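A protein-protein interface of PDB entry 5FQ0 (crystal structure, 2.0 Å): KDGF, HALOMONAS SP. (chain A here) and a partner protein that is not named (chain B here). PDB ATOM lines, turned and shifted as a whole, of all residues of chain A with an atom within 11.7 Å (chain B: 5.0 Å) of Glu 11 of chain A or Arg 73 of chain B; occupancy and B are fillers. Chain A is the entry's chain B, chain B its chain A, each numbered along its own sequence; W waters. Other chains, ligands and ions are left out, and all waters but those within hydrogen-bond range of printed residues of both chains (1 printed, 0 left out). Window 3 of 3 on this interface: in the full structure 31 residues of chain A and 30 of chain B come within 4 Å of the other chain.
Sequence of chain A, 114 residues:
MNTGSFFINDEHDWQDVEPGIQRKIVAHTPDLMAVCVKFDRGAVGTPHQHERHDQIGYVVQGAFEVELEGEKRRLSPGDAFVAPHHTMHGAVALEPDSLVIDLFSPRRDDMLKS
Water W1 bridges NH2 of Arg 73 of chain B (3.4 Å) and OE2 of Glu 11 of chain A (3.4 Å).
Of the 8 printed residues of chain B, 4 touch a printed residue of chain A.
Among the printed residues, 7 pairs touch across the chains.
Of the printed residues of chain B, Phe 6 of chain A touches Val 66, Glu 71, Arg 73 and Leu 75.
Phe 7 of chain A touches none of the printed residues of chain B.
Printed residues of chain B within 4 Å of Ile 8 of chain A: Arg 73 and Leu 75.
Glu 11 of chain A touches just one residue of chain B: Arg 73.
No residue of chain A comes within 4 Å of Glu 65 of chain B.
Of the printed residues of chain A, Glu 71 of chain B touches Phe 6 (3.3 Å).
Of chain A, only Phe 6, Ile 8 and Glu 11 come within 4 Å of Arg 73 of chain B.
Arg 74 of chain B touches none of the printed residues of chain A.
The nearest residue of chain A that does not touch Arg 73 of chain B is Phe 7 of chain A (6.2 Å).
The nearest printed residue of chain B that does not touch Ile 8 of chain A is Arg 74 of chain B (4.3 Å).
OE2 of Glu 11 of chain A lies within salt-bridge range of NH2 of Arg 73 of chain B.
The backbone carbonyl oxygen of Phe 64 of chain B lies within hydrogen-bond range of the backbone NH of Leu 75 of chain B, at 2.7 Å.
The backbone NH of Val 66 of chain B lies within hydrogen-bond range of the backbone carbonyl oxygen of Arg 73 of chain B.
CZ of Phe 6 of chain A touches O of Val 66 of chain B (3.6 Å).
Glu 71 of chain B touches Phe 6 of chain A.
Phe 6 of chain A touches Arg 73 of chain B.
Phe 6 of chain A touches Leu 75 of chain B (CD1 to CD2, 3.8 Å).
Ile 8 of chain A touches Arg 73 of chain B (CG1 to NH2, 3.5 Å).
Leu 75 of chain B touches Ile 8 of chain A (CD2 to CD1, 3.6 Å).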
ATOM      1  N   GLY A   4      19.113  12.635 -20.682  1.00  0.00           N
ATOM      2  CA  GLY A   4      18.786  11.300 -20.053  1.00  0.00           C
ATOM      3  C   GLY A   4      19.829  10.696 -19.119  1.00  0.00           C
ATOM      4  O   GLY A   4      21.010  11.048 -19.173  1.00  0.00           O
ATOM      5  N   SER A   5      19.410   9.769 -18.254  1.00  0.00           N
ATOM      6  CA  SER A   5      20.332   9.189 -17.280  1.00  0.00           C
ATOM      7  C   SER A   5      19.880   7.768 -16.881  1.00  0.00           C
ATOM      8  O   SER A   5      18.690   7.418 -17.016  1.00  0.00           O
ATOM      9  CB  SER A   5      20.417  10.135 -16.064  1.00  0.00           C
ATOM     10  OG  SER A   5      21.482   9.773 -15.222  1.00  0.00           O
ATOM     11  N   PHE A   6      20.825   6.936 -16.453  1.00  0.00           N
ATOM     12  CA  PHE A   6      20.524   5.554 -16.005  1.00  0.00           C
ATOM     13  C   PHE A   6      20.746   5.432 -14.521  1.00  0.00           C
ATOM     14  O   PHE A   6      21.581   6.115 -13.960  1.00  0.00           O
ATOM     15  CB  PHE A   6      21.414   4.499 -16.707  1.00  0.00           C
ATOM     16  CG  PHE A   6      21.116   4.340 -18.191  1.00  0.00           C
ATOM     17  CD1 PHE A   6      19.990   3.637 -18.622  1.00  0.00           C
ATOM     18  CD2 PHE A   6      21.951   4.920 -19.147  1.00  0.00           C
ATOM     19  CE1 PHE A   6      19.707   3.495 -19.980  1.00  0.00           C
ATOM     20  CE2 PHE A   6      21.676   4.779 -20.505  1.00  0.00           C
ATOM     21  CZ  PHE A   6      20.564   4.065 -20.924  1.00  0.00           C
ATOM     22  N   PHE A   7      20.015   4.541 -13.881  1.00  0.00           N
ATOM     23  CA  PHE A   7      20.294   4.281 -12.473  1.00  0.00           C
ATOM     24  C   PHE A   7      20.573   2.796 -12.412  1.00  0.00           C
ATOM     25  O   PHE A   7      19.726   1.987 -12.829  1.00  0.00           O
ATOM     26  CB  PHE A   7      19.066   4.624 -11.596  1.00  0.00           C
ATOM     27  CG  PHE A   7      19.204   4.171 -10.148  1.00  0.00           C
ATOM     28  CD1 PHE A   7      19.957   4.911  -9.237  1.00  0.00           C
ATOM     29  CD2 PHE A   7      18.572   3.008  -9.703  1.00  0.00           C
ATOM     30  CE1 PHE A   7      20.074   4.508  -7.915  1.00  0.00           C
ATOM     31  CE2 PHE A   7      18.695   2.587  -8.368  1.00  0.00           C
ATOM     32  CZ  PHE A   7      19.431   3.343  -7.484  1.00  0.00           C
ATOM     33  N   ILE A   8      21.761   2.443 -11.930  1.00  0.00           N
ATOM     34  CA  ILE A   8      22.135   1.062 -11.786  1.00  0.00           C
ATOM     35  C   ILE A   8      22.203   0.802 -10.281  1.00  0.00           C
ATOM     36  O   ILE A   8      23.095   1.303  -9.551  1.00  0.00           O
ATOM     37  CB  ILE A   8      23.478   0.738 -12.466  1.00  0.00           C
ATOM     38  CG1 ILE A   8      23.461   1.135 -13.964  1.00  0.00           C
ATOM     39  CG2 ILE A   8      23.830  -0.756 -12.284  1.00  0.00           C
ATOM     40  CD1 ILE A   8      22.339   0.525 -14.791  1.00  0.00           C
ATOM     41  N   ASN A   9      21.253   0.019  -9.815  1.00  0.00           N
ATOM     42  CA  ASN A   9      21.107  -0.177  -8.384  1.00  0.00           C
ATOM     43  C   ASN A   9      22.384  -0.668  -7.715  1.00  0.00           C
ATOM     44  O   ASN A   9      22.720  -0.201  -6.654  1.00  0.00           O
ATOM     45  CB  ASN A   9      19.990  -1.157  -8.141  1.00  0.00           C
ATOM     46  CG  ASN A   9      19.639  -1.295  -6.678  1.00  0.00           C
ATOM     47  OD1 ASN A   9      19.504  -0.319  -5.947  1.00  0.00           O
ATOM     48  ND2 ASN A   9      19.493  -2.519  -6.248  1.00  0.00           N
ATOM     49  N   ASP A  10      23.097  -1.606  -8.351  1.00  0.00           N
ATOM     50  CA  ASP A  10      24.343  -2.139  -7.799  1.00  0.00           C
ATOM     51  C   ASP A  10      25.467  -1.118  -7.692  1.00  0.00           C
ATOM     52  O   ASP A  10      26.489  -1.418  -7.078  1.00  0.00           O
ATOM     53  CB  ASP A  10      24.843  -3.304  -8.645  1.00  0.00           C
ATOM     54  CG  ASP A  10      23.918  -4.511  -8.583  1.00  0.00           C
ATOM     55  OD1 ASP A  10      23.118  -4.657  -7.603  1.00  0.00           O
ATOM     56  OD2 ASP A  10      23.982  -5.311  -9.543  1.00  0.00           O
ATOM     57  N   GLU A  11      25.298   0.084  -8.264  1.00  0.00           N
ATOM     58  CA  GLU A  11      26.347   1.088  -8.190  1.00  0.00           C
ATOM     59  C   GLU A  11      26.118   2.082  -7.064  1.00  0.00           C
ATOM     60  O   GLU A  11      26.981   2.930  -6.836  1.00  0.00           O
ATOM     61  CB  GLU A  11      26.492   1.861  -9.521  1.00  0.00           C
ATOM     62  CG  GLU A  11      26.912   0.973 -10.686  1.00  0.00           C
ATOM     63  CD  GLU A  11      26.921   1.723 -12.019  1.00  0.00           C
ATOM     64  OE1 GLU A  11      26.719   2.964 -12.041  1.00  0.00           O
ATOM     65  OE2 GLU A  11      27.105   1.053 -13.052  1.00  0.00           O
ATOM     66  N   HIS A  12      24.999   1.970  -6.346  1.00  0.00           N
ATOM     67  CA  HIS A  12      24.628   2.953  -5.310  1.00  0.00           C
ATOM     68  C   HIS A  12      24.413   2.338  -3.921  1.00  0.00           C
ATOM     69  O   HIS A  12      23.807   1.284  -3.799  1.00  0.00           O
ATOM     70  CB  HIS A  12      23.357   3.710  -5.734  1.00  0.00           C
ATOM     71  CG  HIS A  12      23.503   4.447  -7.031  1.00  0.00           C
ATOM     72  ND1 HIS A  12      23.855   5.779  -7.093  1.00  0.00           N
ATOM     73  CD2 HIS A  12      23.391   4.024  -8.312  1.00  0.00           C
ATOM     74  CE1 HIS A  12      23.935   6.152  -8.358  1.00  0.00           C
ATOM     75  NE2 HIS A  12      23.658   5.105  -9.122  1.00  0.00           N
ATOM     76  N   ASP A  13      24.901   3.020  -2.885  1.00  0.00           N
ATOM     77  CA  ASP A  13      24.730   2.608  -1.485  1.00  0.00           C
ATOM     78  C   ASP A  13      23.367   3.001  -0.954  1.00  0.00           C
ATOM     79  O   ASP A  13      22.810   4.022  -1.384  1.00  0.00           O
ATOM     80  CB  ASP A  13      25.771   3.339  -0.582  1.00  0.00           C
ATOM     81  CG  ASP A  13      27.228   2.990  -0.910  1.00  0.00           C
ATOM     82  OD1 ASP A  13      27.540   1.958  -1.550  1.00  0.00           O
ATOM     83  OD2 ASP A  13      28.086   3.768  -0.464  1.00  0.00           O
ATOM     84  N   TRP A  14      22.847   2.259   0.026  1.00  0.00           N
ATOM     85  CA  TRP A  14      21.675   2.740   0.759  1.00  0.00           C
ATOM     86  C   TRP A  14      22.053   3.944   1.624  1.00  0.00           C
ATOM     87  O   TRP A  14      23.150   3.996   2.143  1.00  0.00           O
ATOM     88  CB  TRP A  14      21.101   1.651   1.664  1.00  0.00           C
ATOM     89  CG  TRP A  14      20.513   0.500   0.913  1.00  0.00           C
ATOM     90  CD1 TRP A  14      21.077  -0.713   0.742  1.00  0.00           C
ATOM     91  CD2 TRP A  14      19.248   0.463   0.232  1.00  0.00           C
ATOM     92  NE1 TRP A  14      20.244  -1.518  -0.008  1.00  0.00           N
ATOM     93  CE2 TRP A  14      19.115  -0.819  -0.329  1.00  0.00           C
ATOM     94  CE3 TRP A  14      18.216   1.381   0.052  1.00  0.00           C
ATOM     95  CZ2 TRP A  14      17.974  -1.213  -1.074  1.00  0.00           C
ATOM     96  CZ3 TRP A  14      17.079   0.994  -0.697  1.00  0.00           C
ATOM     97  CH2 TRP A  14      16.981  -0.277  -1.247  1.00  0.00           C
ATOM     98  N   GLN A  15      21.130   4.896   1.759  1.00  0.00           N
ATOM     99  CA  GLN A  15      21.319   6.100   2.566  1.00  0.00           C
ATOM    100  C   GLN A  15      20.353   6.006   3.736  1.00  0.00           C
ATOM    101  O   GLN A  15      19.185   5.693   3.532  1.00  0.00           O
ATOM    102  CB  GLN A  15      20.984   7.374   1.751  1.00  0.00           C
ATOM    103  CG  GLN A  15      21.812   7.586   0.483  1.00  0.00           C
ATOM    104  CD  GLN A  15      23.307   7.642   0.774  1.00  0.00           C
ATOM    105  OE1 GLN A  15      23.740   8.278   1.739  1.00  0.00           O
ATOM    106  NE2 GLN A  15      24.101   6.927  -0.026  1.00  0.00           N
ATOM    107  N   ARG A  23      17.160   4.564   1.978  1.00  0.00           N
ATOM    108  CA  ARG A  23      16.693   4.826   0.626  1.00  0.00           C
ATOM    109  C   ARG A  23      17.791   5.016  -0.373  1.00  0.00           C
ATOM    110  O   ARG A  23      18.936   5.222  -0.011  1.00  0.00           O
ATOM    111  CB  ARG A  23      15.775   6.053   0.579  1.00  0.00           C
ATOM    112  CG  ARG A  23      16.470   7.393   0.665  1.00  0.00           C
ATOM    113  CD  ARG A  23      15.400   8.474   0.546  1.00  0.00           C
ATOM    114  NE  ARG A  23      15.973   9.741   0.952  1.00  0.00           N
ATOM    115  CZ  ARG A  23      15.432  10.588   1.811  1.00  0.00           C
ATOM    116  NH1 ARG A  23      14.239  10.368   2.339  1.00  0.00           N
ATOM    117  NH2 ARG A  23      16.090  11.687   2.105  1.00  0.00           N
ATOM    118  N   LYS A  24      17.421   4.945  -1.636  1.00  0.00           N
ATOM    119  CA  LYS A  24      18.293   5.396  -2.717  1.00  0.00           C
ATOM    120  C   LYS A  24      17.451   6.294  -3.636  1.00  0.00           C
ATOM    121  O   LYS A  24      16.337   5.887  -4.048  1.00  0.00           O
ATOM    122  CB  LYS A  24      18.810   4.224  -3.525  1.00  0.00           C
ATOM    123  CG  LYS A  24      19.554   3.147  -2.733  1.00  0.00           C
ATOM    124  CD  LYS A  24      20.167   2.142  -3.703  1.00  0.00           C
ATOM    125  CE  LYS A  24      20.719   0.912  -2.965  1.00  0.00           C
ATOM    126  NZ  LYS A  24      21.507   0.010  -3.868  1.00  0.00           N
ATOM    127  N   ILE A  25      17.979   7.472  -3.968  1.00  0.00           N
ATOM    128  CA  ILE A  25      17.346   8.355  -4.956  1.00  0.00           C
ATOM    129  C   ILE A  25      17.583   7.705  -6.316  1.00  0.00           C
ATOM    130  O   ILE A  25      18.712   7.563  -6.711  1.00  0.00           O
ATOM    131  CB  ILE A  25      17.989   9.763  -4.991  1.00  0.00           C
ATOM    132  CG1 ILE A  25      18.013  10.412  -3.579  1.00  0.00           C
ATOM    133  CG2 ILE A  25      17.283  10.651  -6.050  1.00  0.00           C
ATOM    134  CD1 ILE A  25      16.657  10.574  -2.967  1.00  0.00           C
ATOM    135  N   VAL A  26      16.530   7.268  -6.991  1.00  0.00           N
ATOM    136  CA  VAL A  26      16.650   6.523  -8.241  1.00  0.00           C
ATOM    137  C   VAL A  26      16.942   7.469  -9.434  1.00  0.00           C
ATOM    138  O   VAL A  26      17.984   7.364 -10.080  1.00  0.00           O
ATOM    139  CB  VAL A  26      15.413   5.601  -8.438  1.00  0.00           C
ATOM    140  CG1 VAL A  26      15.342   5.051  -9.843  1.00  0.00           C
ATOM    141  CG2 VAL A  26      15.453   4.450  -7.405  1.00  0.00           C
ATOM    142  N   PHE B  64      15.923  -5.433 -19.691  1.00  0.00           N
ATOM    143  CA  PHE B  64      15.665  -4.658 -20.892  1.00  0.00           C
ATOM    144  C   PHE B  64      16.994  -4.119 -21.332  1.00  0.00           C
ATOM    145  O   PHE B  64      17.832  -3.787 -20.480  1.00  0.00           O
ATOM    146  CB  PHE B  64      14.746  -3.427 -20.596  1.00  0.00           C
ATOM    147  CG  PHE B  64      13.308  -3.786 -20.296  1.00  0.00           C
ATOM    148  CD1 PHE B  64      12.914  -4.126 -18.992  1.00  0.00           C
ATOM    149  CD2 PHE B  64      12.344  -3.815 -21.313  1.00  0.00           C
ATOM    150  CE1 PHE B  64      11.582  -4.455 -18.716  1.00  0.00           C
ATOM    151  CE2 PHE B  64      11.029  -4.180 -21.039  1.00  0.00           C
ATOM    152  CZ  PHE B  64      10.650  -4.508 -19.740  1.00  0.00           C
ATOM    153  N   GLU B  65      17.208  -4.030 -22.652  1.00  0.00           N
ATOM    154  CA  GLU B  65      18.258  -3.137 -23.116  1.00  0.00           C
ATOM    155  C   GLU B  65      17.558  -1.830 -23.477  1.00  0.00           C
ATOM    156  O   GLU B  65      16.606  -1.835 -24.274  1.00  0.00           O
ATOM    157  CB  GLU B  65      19.066  -3.676 -24.304  1.00  0.00           C
ATOM    158  CG  GLU B  65      19.874  -2.531 -24.902  1.00  0.00           C
ATOM    159  CD  GLU B  65      21.144  -2.949 -25.600  1.00  0.00           C
ATOM    160  OE1 GLU B  65      22.035  -3.492 -24.912  1.00  0.00           O
ATOM    161  OE2 GLU B  65      21.232  -2.697 -26.831  1.00  0.00           O
ATOM    162  N   VAL B  66      17.993  -0.740 -22.854  1.00  0.00           N
ATOM    163  CA  VAL B  66      17.320   0.553 -23.009  1.00  0.00           C
ATOM    164  C   VAL B  66      18.269   1.506 -23.677  1.00  0.00           C
ATOM    165  O   VAL B  66      19.450   1.591 -23.317  1.00  0.00           O
ATOM    166  CB  VAL B  66      16.800   1.190 -21.676  1.00  0.00           C
ATOM    167  CG1 VAL B  66      16.524   2.691 -21.863  1.00  0.00           C
ATOM    168  CG2 VAL B  66      15.514   0.476 -21.220  1.00  0.00           C
ATOM    169  N   GLU B  71      22.781   6.026 -26.475  1.00  0.00           N
ATOM    170  CA  GLU B  71      23.469   5.317 -25.395  1.00  0.00           C
ATOM    171  C   GLU B  71      22.651   4.103 -24.863  1.00  0.00           C
ATOM    172  O   GLU B  71      21.509   4.247 -24.431  1.00  0.00           O
ATOM    173  CB  GLU B  71      23.799   6.331 -24.294  1.00  0.00           C
ATOM    174  CG  GLU B  71      23.802   5.829 -22.862  1.00  0.00           C
ATOM    175  CD  GLU B  71      25.180   5.561 -22.273  1.00  0.00           C
ATOM    176  OE1 GLU B  71      26.014   4.904 -22.942  1.00  0.00           O
ATOM    177  OE2 GLU B  71      25.420   5.990 -21.115  1.00  0.00           O
ATOM    178  N   LYS B  72      23.241   2.916 -24.870  1.00  0.00           N
ATOM    179  CA  LYS B  72      22.522   1.717 -24.430  1.00  0.00           C
ATOM    180  C   LYS B  72      22.966   1.230 -23.063  1.00  0.00           C
ATOM    181  O   LYS B  72      24.139   1.273 -22.703  1.00  0.00           O
ATOM    182  CB  LYS B  72      22.653   0.584 -25.438  1.00  0.00           C
ATOM    183  CG  LYS B  72      22.723   1.065 -26.866  1.00  0.00           C
ATOM    184  CD  LYS B  72      21.759   0.334 -27.789  1.00  0.00           C
ATOM    185  CE  LYS B  72      21.327   1.270 -28.910  1.00  0.00           C
ATOM    186  NZ  LYS B  72      21.579   0.696 -30.253  1.00  0.00           N
ATOM    187  N   ARG B  73      22.020   0.755 -22.285  1.00  0.00           N
ATOM    188  CA  ARG B  73      22.410   0.133 -21.044  1.00  0.00           C
ATOM    189  C   ARG B  73      21.473  -1.042 -20.764  1.00  0.00           C
ATOM    190  O   ARG B  73      20.296  -1.014 -21.166  1.00  0.00           O
ATOM    191  CB  ARG B  73      22.454   1.169 -19.925  1.00  0.00           C
ATOM    192  CG  ARG B  73      23.467   0.845 -18.880  1.00  0.00           C
ATOM    193  CD  ARG B  73      24.786   1.563 -19.079  1.00  0.00           C
ATOM    194  NE  ARG B  73      25.557   1.251 -17.883  1.00  0.00           N
ATOM    195  CZ  ARG B  73      25.735   2.076 -16.853  1.00  0.00           C
ATOM    196  NH1 ARG B  73      25.252   3.316 -16.903  1.00  0.00           N
ATOM    197  NH2 ARG B  73      26.427   1.663 -15.785  1.00  0.00           N
ATOM    198  N   ARG B  74      22.019  -2.097 -20.156  1.00  0.00           N
ATOM    199  CA  ARG B  74      21.210  -3.272 -19.823  1.00  0.00           C
ATOM    200  C   ARG B  74      20.647  -3.005 -18.437  1.00  0.00           C
ATOM    201  O   ARG B  74      21.407  -2.696 -17.516  1.00  0.00           O
ATOM    202  CB  ARG B  74      22.024  -4.571 -19.821  1.00  0.00           C
ATOM    203  CG  ARG B  74      21.110  -5.787 -19.804  1.00  0.00           C
ATOM    204  CD  ARG B  74      21.841  -7.110 -19.608  1.00  0.00           C
ATOM    205  NE  ARG B  74      21.294  -7.738 -18.419  1.00  0.00           N
ATOM    206  CZ  ARG B  74      20.442  -8.753 -18.361  1.00  0.00           C
ATOM    207  NH1 ARG B  74      20.005  -9.390 -19.443  1.00  0.00           N
ATOM    208  NH2 ARG B  74      20.055  -9.151 -17.161  1.00  0.00           N
ATOM    209  N   LEU B  75      19.325  -3.094 -18.287  1.00  0.00           N
ATOM    210  CA  LEU B  75      18.696  -2.769 -16.982  1.00  0.00           C
ATOM    211  C   LEU B  75      17.998  -4.013 -16.456  1.00  0.00           C
ATOM    212  O   LEU B  75      17.232  -4.659 -17.170  1.00  0.00           O
ATOM    213  CB  LEU B  75      17.694  -1.595 -17.117  1.00  0.00           C
ATOM    214  CG  LEU B  75      18.199  -0.267 -17.691  1.00  0.00           C
ATOM    215  CD1 LEU B  75      17.075   0.776 -17.635  1.00  0.00           C
ATOM    216  CD2 LEU B  75      19.482   0.278 -17.000  1.00  0.00           C
HETATM  217  O   HOH W   1      26.193  -1.587 -14.985  1.00  0.00           O
